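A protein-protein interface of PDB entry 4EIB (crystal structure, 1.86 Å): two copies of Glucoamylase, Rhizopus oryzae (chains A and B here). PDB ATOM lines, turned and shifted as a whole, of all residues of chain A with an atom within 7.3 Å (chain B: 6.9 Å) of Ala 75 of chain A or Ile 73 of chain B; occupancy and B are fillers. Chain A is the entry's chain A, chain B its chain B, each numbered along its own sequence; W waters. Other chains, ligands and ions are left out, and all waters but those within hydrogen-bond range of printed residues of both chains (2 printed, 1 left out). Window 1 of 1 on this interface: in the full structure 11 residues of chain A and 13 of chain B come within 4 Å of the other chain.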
ATOM      1  N   ILE A  45      -3.734 -14.776 -10.940  1.00  0.00           N
ATOM      2  CA  ILE A  45      -3.268 -14.327 -12.264  1.00  0.00           C
ATOM      3  C   ILE A  45      -4.429 -13.545 -12.871  1.00  0.00           C
ATOM      4  O   ILE A  45      -5.553 -14.006 -12.800  1.00  0.00           O
ATOM      5  CB  ILE A  45      -2.945 -15.515 -13.193  1.00  0.00           C
ATOM      6  CG1 ILE A  45      -1.875 -16.462 -12.614  1.00  0.00           C
ATOM      7  CG2 ILE A  45      -2.436 -15.015 -14.560  1.00  0.00           C
ATOM      8  CD1 ILE A  45      -1.792 -17.808 -13.397  1.00  0.00           C
ATOM      9  N   LYS A  55      -6.986 -21.580 -21.554  1.00  0.00           N
ATOM     10  CA  LYS A  55      -6.195 -22.521 -20.815  1.00  0.00           C
ATOM     11  C   LYS A  55      -5.027 -21.730 -20.250  1.00  0.00           C
ATOM     12  O   LYS A  55      -4.316 -21.064 -21.001  1.00  0.00           O
ATOM     13  CB  LYS A  55      -5.637 -23.550 -21.751  1.00  0.00           C
ATOM     14  CG  LYS A  55      -4.854 -24.656 -21.050  1.00  0.00           C
ATOM     15  CD  LYS A  55      -4.653 -25.782 -22.079  1.00  0.00           C
ATOM     16  CE  LYS A  55      -3.568 -26.758 -21.652  1.00  0.00           C
ATOM     17  NZ  LYS A  55      -3.017 -27.506 -22.828  1.00  0.00           N
ATOM     18  N   VAL A  56      -4.807 -21.807 -18.952  1.00  0.00           N
ATOM     19  CA  VAL A  56      -3.758 -20.964 -18.359  1.00  0.00           C
ATOM     20  C   VAL A  56      -2.878 -21.877 -17.573  1.00  0.00           C
ATOM     21  O   VAL A  56      -3.395 -22.604 -16.716  1.00  0.00           O
ATOM     22  CB  VAL A  56      -4.359 -19.909 -17.419  1.00  0.00           C
ATOM     23  CG1 VAL A  56      -3.234 -19.079 -16.775  1.00  0.00           C
ATOM     24  CG2 VAL A  56      -5.325 -19.027 -18.205  1.00  0.00           C
ATOM     25  N   THR A  57      -1.566 -21.841 -17.841  1.00  0.00           N
ATOM     26  CA  THR A  57      -0.666 -22.719 -17.140  1.00  0.00           C
ATOM     27  C   THR A  57       0.575 -21.968 -16.633  1.00  0.00           C
ATOM     28  O   THR A  57       0.891 -20.836 -17.122  1.00  0.00           O
ATOM     29  CB  THR A  57      -0.234 -23.918 -18.010  1.00  0.00           C
ATOM     30  OG1 THR A  57       0.324 -23.452 -19.229  1.00  0.00           O
ATOM     31  CG2 THR A  57      -1.402 -24.871 -18.361  1.00  0.00           C
ATOM     32  N   VAL A  58       1.251 -22.566 -15.641  1.00  0.00           N
ATOM     33  CA  VAL A  58       2.444 -21.939 -15.091  1.00  0.00           C
ATOM     34  C   VAL A  58       3.570 -22.902 -15.490  1.00  0.00           C
ATOM     35  O   VAL A  58       3.471 -24.119 -15.246  1.00  0.00           O
ATOM     36  CB  VAL A  58       2.398 -21.739 -13.571  1.00  0.00           C
ATOM     37  CG1 VAL A  58       3.784 -21.224 -13.072  1.00  0.00           C
ATOM     38  CG2 VAL A  58       1.253 -20.778 -13.159  1.00  0.00           C
ATOM     39  N   GLY A  71       8.832 -28.488 -19.354  1.00  0.00           N
ATOM     40  CA  GLY A  71       7.884 -29.562 -19.062  1.00  0.00           C
ATOM     41  C   GLY A  71       7.381 -29.593 -17.624  1.00  0.00           C
ATOM     42  O   GLY A  71       6.637 -30.512 -17.292  1.00  0.00           O
ATOM     43  N   ASN A  72       7.738 -28.610 -16.785  1.00  0.00           N
ATOM     44  CA  ASN A  72       7.266 -28.591 -15.399  1.00  0.00           C
ATOM     45  C   ASN A  72       6.089 -27.645 -15.403  1.00  0.00           C
ATOM     46  O   ASN A  72       6.294 -26.419 -15.572  1.00  0.00           O
ATOM     47  CB  ASN A  72       8.324 -28.055 -14.464  1.00  0.00           C
ATOM     48  CG  ASN A  72       9.610 -28.856 -14.517  1.00  0.00           C
ATOM     49  OD1 ASN A  72      10.703 -28.282 -14.460  1.00  0.00           O
ATOM     50  ND2 ASN A  72       9.503 -30.158 -14.649  1.00  0.00           N
ATOM     51  N   ILE A  73       4.867 -28.193 -15.280  1.00  0.00           N
ATOM     52  CA  ILE A  73       3.671 -27.437 -15.632  1.00  0.00           C
ATOM     53  C   ILE A  73       2.674 -27.558 -14.497  1.00  0.00           C
ATOM     54  O   ILE A  73       2.551 -28.627 -13.878  1.00  0.00           O
ATOM     55  CB  ILE A  73       3.053 -27.941 -16.959  1.00  0.00           C
ATOM     56  CG1 ILE A  73       3.897 -27.443 -18.136  1.00  0.00           C
ATOM     57  CG2 ILE A  73       1.639 -27.377 -17.172  1.00  0.00           C
ATOM     58  CD1 ILE A  73       3.793 -28.350 -19.347  1.00  0.00           C
ATOM     59  N   ILE A  74       2.008 -26.453 -14.192  1.00  0.00           N
ATOM     60  CA  ILE A  74       0.915 -26.395 -13.217  1.00  0.00           C
ATOM     61  C   ILE A  74      -0.242 -25.734 -13.951  1.00  0.00           C
ATOM     62  O   ILE A  74      -0.057 -24.694 -14.589  1.00  0.00           O
ATOM     63  CB  ILE A  74       1.292 -25.527 -11.998  1.00  0.00           C
ATOM     64  CG1 ILE A  74       2.344 -26.261 -11.132  1.00  0.00           C
ATOM     65  CG2 ILE A  74       0.086 -25.271 -11.099  1.00  0.00           C
ATOM     66  CD1 ILE A  74       3.138 -25.290 -10.293  1.00  0.00           C
ATOM     67  N   ALA A  75      -1.438 -26.333 -13.861  1.00  0.00           N
ATOM     68  CA  ALA A  75      -2.646 -25.770 -14.483  1.00  0.00           C
ATOM     69  C   ALA A  75      -3.328 -24.836 -13.533  1.00  0.00           C
ATOM     70  O   ALA A  75      -3.576 -25.171 -12.386  1.00  0.00           O
ATOM     71  CB  ALA A  75      -3.634 -26.874 -14.885  1.00  0.00           C
ATOM     72  N   ALA A  76      -3.689 -23.668 -14.026  1.00  0.00           N
ATOM     73  CA  ALA A  76      -4.550 -22.746 -13.260  1.00  0.00           C
ATOM     74  C   ALA A  76      -6.062 -22.991 -13.494  1.00  0.00           C
ATOM     75  O   ALA A  76      -6.452 -23.611 -14.499  1.00  0.00           O
ATOM     76  CB  ALA A  76      -4.174 -21.335 -13.588  1.00  0.00           C
ATOM     77  N   SER A  77      -6.893 -22.524 -12.545  1.00  0.00           N
ATOM     78  CA  SER A  77      -8.343 -22.649 -12.596  1.00  0.00           C
ATOM     79  C   SER A  77      -8.989 -21.276 -12.565  1.00  0.00           C
ATOM     80  O   SER A  77      -8.521 -20.362 -11.885  1.00  0.00           O
ATOM     81  CB  SER A  77      -8.862 -23.445 -11.394  1.00  0.00           C
ATOM     82  OG  SER A  77      -8.410 -24.815 -11.346  1.00  0.00           O
ATOM     83  N   TRP A  90      -7.675 -15.963 -12.241  1.00  0.00           N
ATOM     84  CA  TRP A  90      -7.356 -17.393 -12.194  1.00  0.00           C
ATOM     85  C   TRP A  90      -6.372 -17.691 -11.077  1.00  0.00           C
ATOM     86  O   TRP A  90      -5.491 -16.890 -10.783  1.00  0.00           O
ATOM     87  CB  TRP A  90      -6.784 -17.866 -13.527  1.00  0.00           C
ATOM     88  CG  TRP A  90      -7.808 -17.894 -14.655  1.00  0.00           C
ATOM     89  CD1 TRP A  90      -8.601 -16.846 -15.106  1.00  0.00           C
ATOM     90  CD2 TRP A  90      -8.112 -19.021 -15.547  1.00  0.00           C
ATOM     91  NE1 TRP A  90      -9.362 -17.235 -16.163  1.00  0.00           N
ATOM     92  CE2 TRP A  90      -9.127 -18.531 -16.484  1.00  0.00           C
ATOM     93  CE3 TRP A  90      -7.667 -20.355 -15.646  1.00  0.00           C
ATOM     94  CZ2 TRP A  90      -9.710 -19.358 -17.472  1.00  0.00           C
ATOM     95  CZ3 TRP A  90      -8.258 -21.175 -16.634  1.00  0.00           C
ATOM     96  CH2 TRP A  90      -9.249 -20.671 -17.543  1.00  0.00           C
ATOM     97  N   THR A  91      -6.501 -18.845 -10.448  1.00  0.00           N
ATOM     98  CA  THR A  91      -5.628 -19.175  -9.305  1.00  0.00           C
ATOM     99  C   THR A  91      -4.956 -20.489  -9.602  1.00  0.00           C
ATOM    100  O   THR A  91      -5.432 -21.268 -10.435  1.00  0.00           O
ATOM    101  CB  THR A  91      -6.406 -19.346  -7.975  1.00  0.00           C
ATOM    102  OG1 THR A  91      -7.503 -20.193  -8.219  1.00  0.00           O
ATOM    103  CG2 THR A  91      -6.954 -17.973  -7.452  1.00  0.00           C
ATOM    104  N   PHE A  92      -3.871 -20.762  -8.873  1.00  0.00           N
ATOM    105  CA  PHE A  92      -3.216 -22.029  -8.970  1.00  0.00           C
ATOM    106  C   PHE A  92      -2.642 -22.381  -7.631  1.00  0.00           C
ATOM    107  O   PHE A  92      -2.405 -21.525  -6.803  1.00  0.00           O
ATOM    108  CB  PHE A  92      -2.100 -22.038 -10.051  1.00  0.00           C
ATOM    109  CG  PHE A  92      -0.939 -21.081  -9.773  1.00  0.00           C
ATOM    110  CD1 PHE A  92      -0.976 -19.730 -10.192  1.00  0.00           C
ATOM    111  CD2 PHE A  92       0.213 -21.538  -9.113  1.00  0.00           C
ATOM    112  CE1 PHE A  92       0.087 -18.865  -9.946  1.00  0.00           C
ATOM    113  CE2 PHE A  92       1.296 -20.642  -8.857  1.00  0.00           C
ATOM    114  CZ  PHE A  92       1.227 -19.314  -9.294  1.00  0.00           C
ATOM    115  N   SER A  93      -2.481 -23.668  -7.393  1.00  0.00           N
ATOM    116  CA  SER A  93      -1.828 -24.086  -6.180  1.00  0.00           C
ATOM    117  C   SER A  93      -1.341 -25.542  -6.397  1.00  0.00           C
ATOM    118  O   SER A  93      -2.158 -26.395  -6.824  1.00  0.00           O
ATOM    119  CB  SER A  93      -2.823 -24.033  -5.000  1.00  0.00           C
ATOM    120  OG  SER A  93      -2.162 -24.622  -3.877  1.00  0.00           O
ATOM    121  N   ALA A  94      -0.087 -25.853  -6.052  1.00  0.00           N
ATOM    122  CA  ALA A  94       0.465 -27.215  -6.293  1.00  0.00           C
ATOM    123  C   ALA A  94       1.548 -27.493  -5.269  1.00  0.00           C
ATOM    124  O   ALA A  94       2.268 -26.556  -4.849  1.00  0.00           O
ATOM    125  CB  ALA A  94       1.101 -27.328  -7.696  1.00  0.00           C
ATOM    126  N   LYS B  55       6.680 -36.232  -7.313  1.00  0.00           N
ATOM    127  CA  LYS B  55       5.956 -35.351  -8.173  1.00  0.00           C
ATOM    128  C   LYS B  55       4.878 -36.194  -8.868  1.00  0.00           C
ATOM    129  O   LYS B  55       5.185 -37.220  -9.435  1.00  0.00           O
ATOM    130  CB  LYS B  55       6.889 -34.799  -9.216  1.00  0.00           C
ATOM    131  CG  LYS B  55       6.236 -33.753 -10.076  1.00  0.00           C
ATOM    132  CD  LYS B  55       7.313 -33.116 -10.959  1.00  0.00           C
ATOM    133  CE  LYS B  55       6.744 -32.677 -12.297  1.00  0.00           C
ATOM    134  NZ  LYS B  55       7.771 -31.939 -13.113  1.00  0.00           N
ATOM    135  N   THR B  57       1.662 -36.085 -11.607  1.00  0.00           N
ATOM    136  CA  THR B  57       0.934 -35.319 -12.574  1.00  0.00           C
ATOM    137  C   THR B  57      -0.086 -36.154 -13.358  1.00  0.00           C
ATOM    138  O   THR B  57       0.033 -37.412 -13.439  1.00  0.00           O
ATOM    139  CB  THR B  57       1.903 -34.561 -13.540  1.00  0.00           C
ATOM    140  OG1 THR B  57       2.741 -35.481 -14.214  1.00  0.00           O
ATOM    141  CG2 THR B  57       2.868 -33.584 -12.794  1.00  0.00           C
ATOM    142  N   VAL B  58      -1.069 -35.452 -13.948  1.00  0.00           N
ATOM    143  CA  VAL B  58      -2.096 -36.110 -14.785  1.00  0.00           C
ATOM    144  C   VAL B  58      -1.823 -35.609 -16.210  1.00  0.00           C
ATOM    145  O   VAL B  58      -1.728 -34.383 -16.443  1.00  0.00           O
ATOM    146  CB  VAL B  58      -3.523 -35.807 -14.317  1.00  0.00           C
ATOM    147  CG1 VAL B  58      -4.587 -36.436 -15.247  1.00  0.00           C
ATOM    148  CG2 VAL B  58      -3.735 -36.241 -12.856  1.00  0.00           C
ATOM    149  N   VAL B  59      -1.603 -36.544 -17.136  1.00  0.00           N
ATOM    150  CA  VAL B  59      -1.359 -36.206 -18.535  1.00  0.00           C
ATOM    151  C   VAL B  59      -2.646 -36.562 -19.334  1.00  0.00           C
ATOM    152  O   VAL B  59      -3.143 -37.687 -19.195  1.00  0.00           O
ATOM    153  CB  VAL B  59      -0.145 -37.014 -19.028  1.00  0.00           C
ATOM    154  CG1 VAL B  59       0.172 -36.707 -20.491  1.00  0.00           C
ATOM    155  CG2 VAL B  59       1.107 -36.753 -18.121  1.00  0.00           C
ATOM    156  N   TYR B  60      -3.206 -35.668 -20.164  1.00  0.00           N
ATOM    157  CA  TYR B  60      -4.524 -35.985 -20.702  1.00  0.00           C
ATOM    158  C   TYR B  60      -4.669 -35.572 -22.128  1.00  0.00           C
ATOM    159  O   TYR B  60      -3.903 -34.763 -22.617  1.00  0.00           O
ATOM    160  CB  TYR B  60      -5.641 -35.338 -19.871  1.00  0.00           C
ATOM    161  CG  TYR B  60      -5.632 -33.774 -19.863  1.00  0.00           C
ATOM    162  CD1 TYR B  60      -4.829 -33.039 -18.948  1.00  0.00           C
ATOM    163  CD2 TYR B  60      -6.444 -33.042 -20.757  1.00  0.00           C
ATOM    164  CE1 TYR B  60      -4.848 -31.616 -18.954  1.00  0.00           C
ATOM    165  CE2 TYR B  60      -6.459 -31.655 -20.750  1.00  0.00           C
ATOM    166  CZ  TYR B  60      -5.674 -30.954 -19.866  1.00  0.00           C
ATOM    167  OH  TYR B  60      -5.748 -29.558 -19.934  1.00  0.00           O
ATOM    168  N   ASN B  70       1.758 -35.215 -25.391  1.00  0.00           N
ATOM    169  CA  ASN B  70       1.796 -35.464 -23.922  1.00  0.00           C
ATOM    170  C   ASN B  70       2.079 -34.190 -23.112  1.00  0.00           C
ATOM    171  O   ASN B  70       2.725 -34.214 -22.029  1.00  0.00           O
ATOM    172  CB  ASN B  70       2.783 -36.620 -23.572  1.00  0.00           C
ATOM    173  CG  ASN B  70       2.376 -37.940 -24.210  1.00  0.00           C
ATOM    174  OD1 ASN B  70       3.234 -38.817 -24.447  1.00  0.00           O
ATOM    175  ND2 ASN B  70       1.079 -38.111 -24.477  1.00  0.00           N
ATOM    176  N   GLY B  71       1.535 -33.087 -23.611  1.00  0.00           N
ATOM    177  CA  GLY B  71       1.822 -31.764 -23.110  1.00  0.00           C
ATOM    178  C   GLY B  71       0.687 -31.152 -22.322  1.00  0.00           C
ATOM    179  O   GLY B  71       0.879 -30.046 -21.837  1.00  0.00           O
ATOM    180  N   ASN B  72      -0.450 -31.847 -22.148  1.00  0.00           N
ATOM    181  CA  ASN B  72      -1.577 -31.288 -21.417  1.00  0.00           C
ATOM    182  C   ASN B  72      -1.442 -31.898 -20.040  1.00  0.00           C
ATOM    183  O   ASN B  72      -1.666 -33.139 -19.888  1.00  0.00           O
ATOM    184  CB  ASN B  72      -2.930 -31.732 -22.021  1.00  0.00           C
ATOM    185  CG  ASN B  72      -3.075 -31.376 -23.497  1.00  0.00           C
ATOM    186  OD1 ASN B  72      -3.671 -32.130 -24.263  1.00  0.00           O
ATOM    187  ND2 ASN B  72      -2.569 -30.233 -23.896  1.00  0.00           N
ATOM    188  N   ILE B  73      -1.081 -31.070 -19.051  1.00  0.00           N
ATOM    189  CA  ILE B  73      -0.552 -31.570 -17.761  1.00  0.00           C
ATOM    190  C   ILE B  73      -1.334 -30.891 -16.635  1.00  0.00           C
ATOM    191  O   ILE B  73      -1.573 -29.670 -16.686  1.00  0.00           O
ATOM    192  CB  ILE B  73       0.965 -31.210 -17.582  1.00  0.00           C
ATOM    193  CG1 ILE B  73       1.866 -31.840 -18.657  1.00  0.00           C
ATOM    194  CG2 ILE B  73       1.498 -31.719 -16.248  1.00  0.00           C
ATOM    195  CD1 ILE B  73       1.849 -33.323 -18.504  1.00  0.00           C
ATOM    196  N   ILE B  74      -1.707 -31.655 -15.608  1.00  0.00           N
ATOM    197  CA  ILE B  74      -2.290 -31.119 -14.408  1.00  0.00           C
ATOM    198  C   ILE B  74      -1.418 -31.643 -13.280  1.00  0.00           C
ATOM    199  O   ILE B  74      -1.060 -32.824 -13.270  1.00  0.00           O
ATOM    200  CB  ILE B  74      -3.727 -31.619 -14.236  1.00  0.00           C
ATOM    201  CG1 ILE B  74      -4.646 -30.866 -15.226  1.00  0.00           C
ATOM    202  CG2 ILE B  74      -4.274 -31.357 -12.824  1.00  0.00           C
ATOM    203  CD1 ILE B  74      -5.956 -31.575 -15.411  1.00  0.00           C
ATOM    204  N   ALA B  75      -1.042 -30.768 -12.364  1.00  0.00           N
ATOM    205  CA  ALA B  75      -0.196 -31.161 -11.214  1.00  0.00           C
ATOM    206  C   ALA B  75      -1.095 -31.504 -10.035  1.00  0.00           C
ATOM    207  O   ALA B  75      -2.025 -30.756  -9.711  1.00  0.00           O
ATOM    208  CB  ALA B  75       0.761 -30.015 -10.825  1.00  0.00           C
ATOM    209  N   SER B  93      -7.254 -30.868  -9.184  1.00  0.00           N
ATOM    210  CA  SER B  93      -8.471 -30.244  -9.662  1.00  0.00           C
ATOM    211  C   SER B  93      -8.070 -29.093 -10.596  1.00  0.00           C
ATOM    212  O   SER B  93      -7.288 -28.221 -10.187  1.00  0.00           O
ATOM    213  CB  SER B  93      -9.309 -29.691  -8.496  1.00  0.00           C
ATOM    214  OG  SER B  93     -10.440 -29.033  -9.040  1.00  0.00           O
ATOM    215  N   ALA B  94      -8.656 -29.049 -11.794  1.00  0.00           N
ATOM    216  CA  ALA B  94      -8.340 -27.986 -12.743  1.00  0.00           C
ATOM    217  C   ALA B  94      -9.543 -27.689 -13.646  1.00  0.00           C
ATOM    218  O   ALA B  94     -10.345 -28.588 -13.962  1.00  0.00           O
ATOM    219  CB  ALA B  94      -7.119 -28.338 -13.591  1.00  0.00           C
ATOM    220  N   SER B  95      -9.644 -26.424 -14.080  1.00  0.00           N
ATOM    221  CA  SER B  95     -10.647 -26.028 -15.095  1.00  0.00           C
ATOM    222  C   SER B  95     -10.183 -26.660 -16.389  1.00  0.00           C
ATOM    223  O   SER B  95      -9.040 -26.450 -16.802  1.00  0.00           O
ATOM    224  CB  SER B  95     -10.676 -24.488 -15.295  1.00  0.00           C
ATOM    225  OG  SER B  95     -11.013 -23.746 -14.116  1.00  0.00           O
ATOM    226  N   VAL B  96     -11.027 -27.475 -17.022  1.00  0.00           N
ATOM    227  CA  VAL B  96     -10.629 -28.116 -18.282  1.00  0.00           C
ATOM    228  C   VAL B  96     -11.769 -27.987 -19.271  1.00  0.00           C
ATOM    229  O   VAL B  96     -12.914 -28.260 -18.897  1.00  0.00           O
ATOM    230  CB  VAL B  96     -10.251 -29.606 -18.007  1.00  0.00           C
ATOM    231  CG1 VAL B  96     -10.351 -30.415 -19.258  1.00  0.00           C
ATOM    232  CG2 VAL B  96      -8.861 -29.682 -17.355  1.00  0.00           C
ATOM    233  N   TYR B 103      -3.714 -40.427 -18.191  1.00  0.00           N
ATOM    234  CA  TYR B 103      -2.991 -41.345 -17.353  1.00  0.00           C
ATOM    235  C   TYR B 103      -2.244 -40.536 -16.291  1.00  0.00           C
ATOM    236  O   TYR B 103      -2.177 -39.278 -16.367  1.00  0.00           O
ATOM    237  CB  TYR B 103      -2.030 -42.228 -18.207  1.00  0.00           C
ATOM    238  CG  TYR B 103      -0.921 -41.486 -18.980  1.00  0.00           C
ATOM    239  CD1 TYR B 103       0.291 -41.130 -18.350  1.00  0.00           C
ATOM    240  CD2 TYR B 103      -1.065 -41.169 -20.342  1.00  0.00           C
ATOM    241  CE1 TYR B 103       1.342 -40.482 -19.059  1.00  0.00           C
ATOM    242  CE2 TYR B 103      -0.019 -40.540 -21.055  1.00  0.00           C
ATOM    243  CZ  TYR B 103       1.179 -40.191 -20.399  1.00  0.00           C
ATOM    244  OH  TYR B 103       2.185 -39.559 -21.094  1.00  0.00           O
ATOM    245  N   LYS B 105       1.292 -39.869 -13.904  1.00  0.00           N
ATOM    246  CA  LYS B 105       2.745 -40.011 -13.979  1.00  0.00           C
ATOM    247  C   LYS B 105       3.282 -39.657 -12.583  1.00  0.00           C
ATOM    248  O   LYS B 105       2.828 -38.672 -11.969  1.00  0.00           O
ATOM    249  CB  LYS B 105       3.316 -39.099 -15.054  1.00  0.00           C
ATOM    250  CG  LYS B 105       4.853 -39.154 -15.180  1.00  0.00           C
ATOM    251  CD  LYS B 105       5.288 -38.159 -16.281  1.00  0.00           C
ATOM    252  CE  LYS B 105       6.800 -38.008 -16.358  1.00  0.00           C
ATOM    253  NZ  LYS B 105       7.194 -36.922 -17.311  1.00  0.00           N
HETATM  254  O   HOH W   1      -4.876 -27.753 -10.956  1.00  0.00           O
HETATM  255  O   HOH W   2      -0.561 -28.023 -20.690  1.00  0.00           O
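Lys 55 of chain A touches Asn 72 of chain B, and with the chains exchanged Asn 72 of chain A touches Lys 55 of chain B.
Ile 73 of chain A touches its own counterpart, Ile 73 of chain B.
Ile 73 of chain A touches Ala 75 of chain B, and with the chains exchanged Ala 75 of chain A touches Ile 73 of chain B.
Ala 75 of chain A touches Ala 94 of chain B, but with the chains exchanged Ala 94 of chain A does not touch Ala 75 of chain B (4.1 Å).
Of the 10 pairs that touch across the chains among the printed residues, 5 have their exchanged pair printed and touching as well.
The backbone NH (N) of Ser 77 of chain A sits at hydrogen-bond distance from the backbone carbonyl oxygen (O) of Thr 91 of chain A, 2.9 Å away.
N of Tyr 60 of chain B is in hydrogen-bond range of O of Asn 72 of chain B (3.0 Å).
Water W1 lies within hydrogen-bond range of O of Ser 93 of chain B (2.6 Å) and O of Ala 75 of chain A (3.2 Å).
Water W2 lies within hydrogen-bond range of O of Gly 71 of chain B (2.7 Å), NZ of Lys 55 of chain A (3.3 Å) and N of Ile 73 of chain B (3.5 Å).
NZ of Lys 55 of chain A sits close to ND2 of Asn 72 of chain B (3.0 Å).
The side-chain amino group of Lys 55 of chain B lies close to the side-chain amide nitrogen of Asn 72 of chain A, 2.9 Å away.
The side-chain hydroxyl of Ser 77 of chain A sits at hydrogen-bond distance from the backbone NH of Ser 95 of chain B, at 3.4 Å.
Of the printed residues of chain B, Ala 75 of chain A touches Ile 73 and Ala 94.
Of the printed residues of chain A, Ile 73 of chain B touches Ile 73 (3.9 Å) and Ala 75 (3.9 Å).
Printed residues of chain A within 4 Å of Lys 55 of chain B: Asn 72.
Of the printed residues of chain A, Ser 95 of chain B touches Ser 77 (3.3 Å).
Printed residues of chain B within 4 Å of Lys 55 of chain A: Tyr 60 and Asn 72.
Of the printed residues of chain A, Tyr 60 of chain B touches Lys 55.
Printed residues of chain A within 4 Å of Ser 93 of chain B: Ser 77.
Among the printed residues, merely in contact across the chains: Lys 55 of chain A with Tyr 60 of chain B (3.9 Å), Ile 73 of chain A with Ile 73 of chain B (3.9 Å), Ile 73 of chain A with Ala 75 of chain B (3.8 Å), Ala 75 of chain A with Ile 73 of chain B (3.9 Å), Ala 75 of chain A with Ala 94 of chain B (3.995 Å), Ser 77 of chain A with Ser 93 of chain B (3.8 Å) and Ser 77 of chain A with Ala 94 of chain B (3.5 Å).
Of the 17 printed residues of chain B, 8 touch a printed residue of chain A.
Printed residues of chain B that touch a printed residue of chain A: Lys 55, Tyr 60, Asn 72, Ile 73, Ala 75, Ser 93, Ala 94 and Ser 95.
Hydrophobic or aromatic side chains of chain B that line the printed part of chain A: Tyr 60, Ile 73, Ala 75 and Ala 94.
Along chain B the printed residues that touch a printed residue of chain A span positions 55 to 95.
Among the printed residues, 10 pairs touch across the chains.
Among the printed residues, no Asp or Glu carboxylate lies within 4 Å of a Lys or Arg side-chain nitrogen of the other chain.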
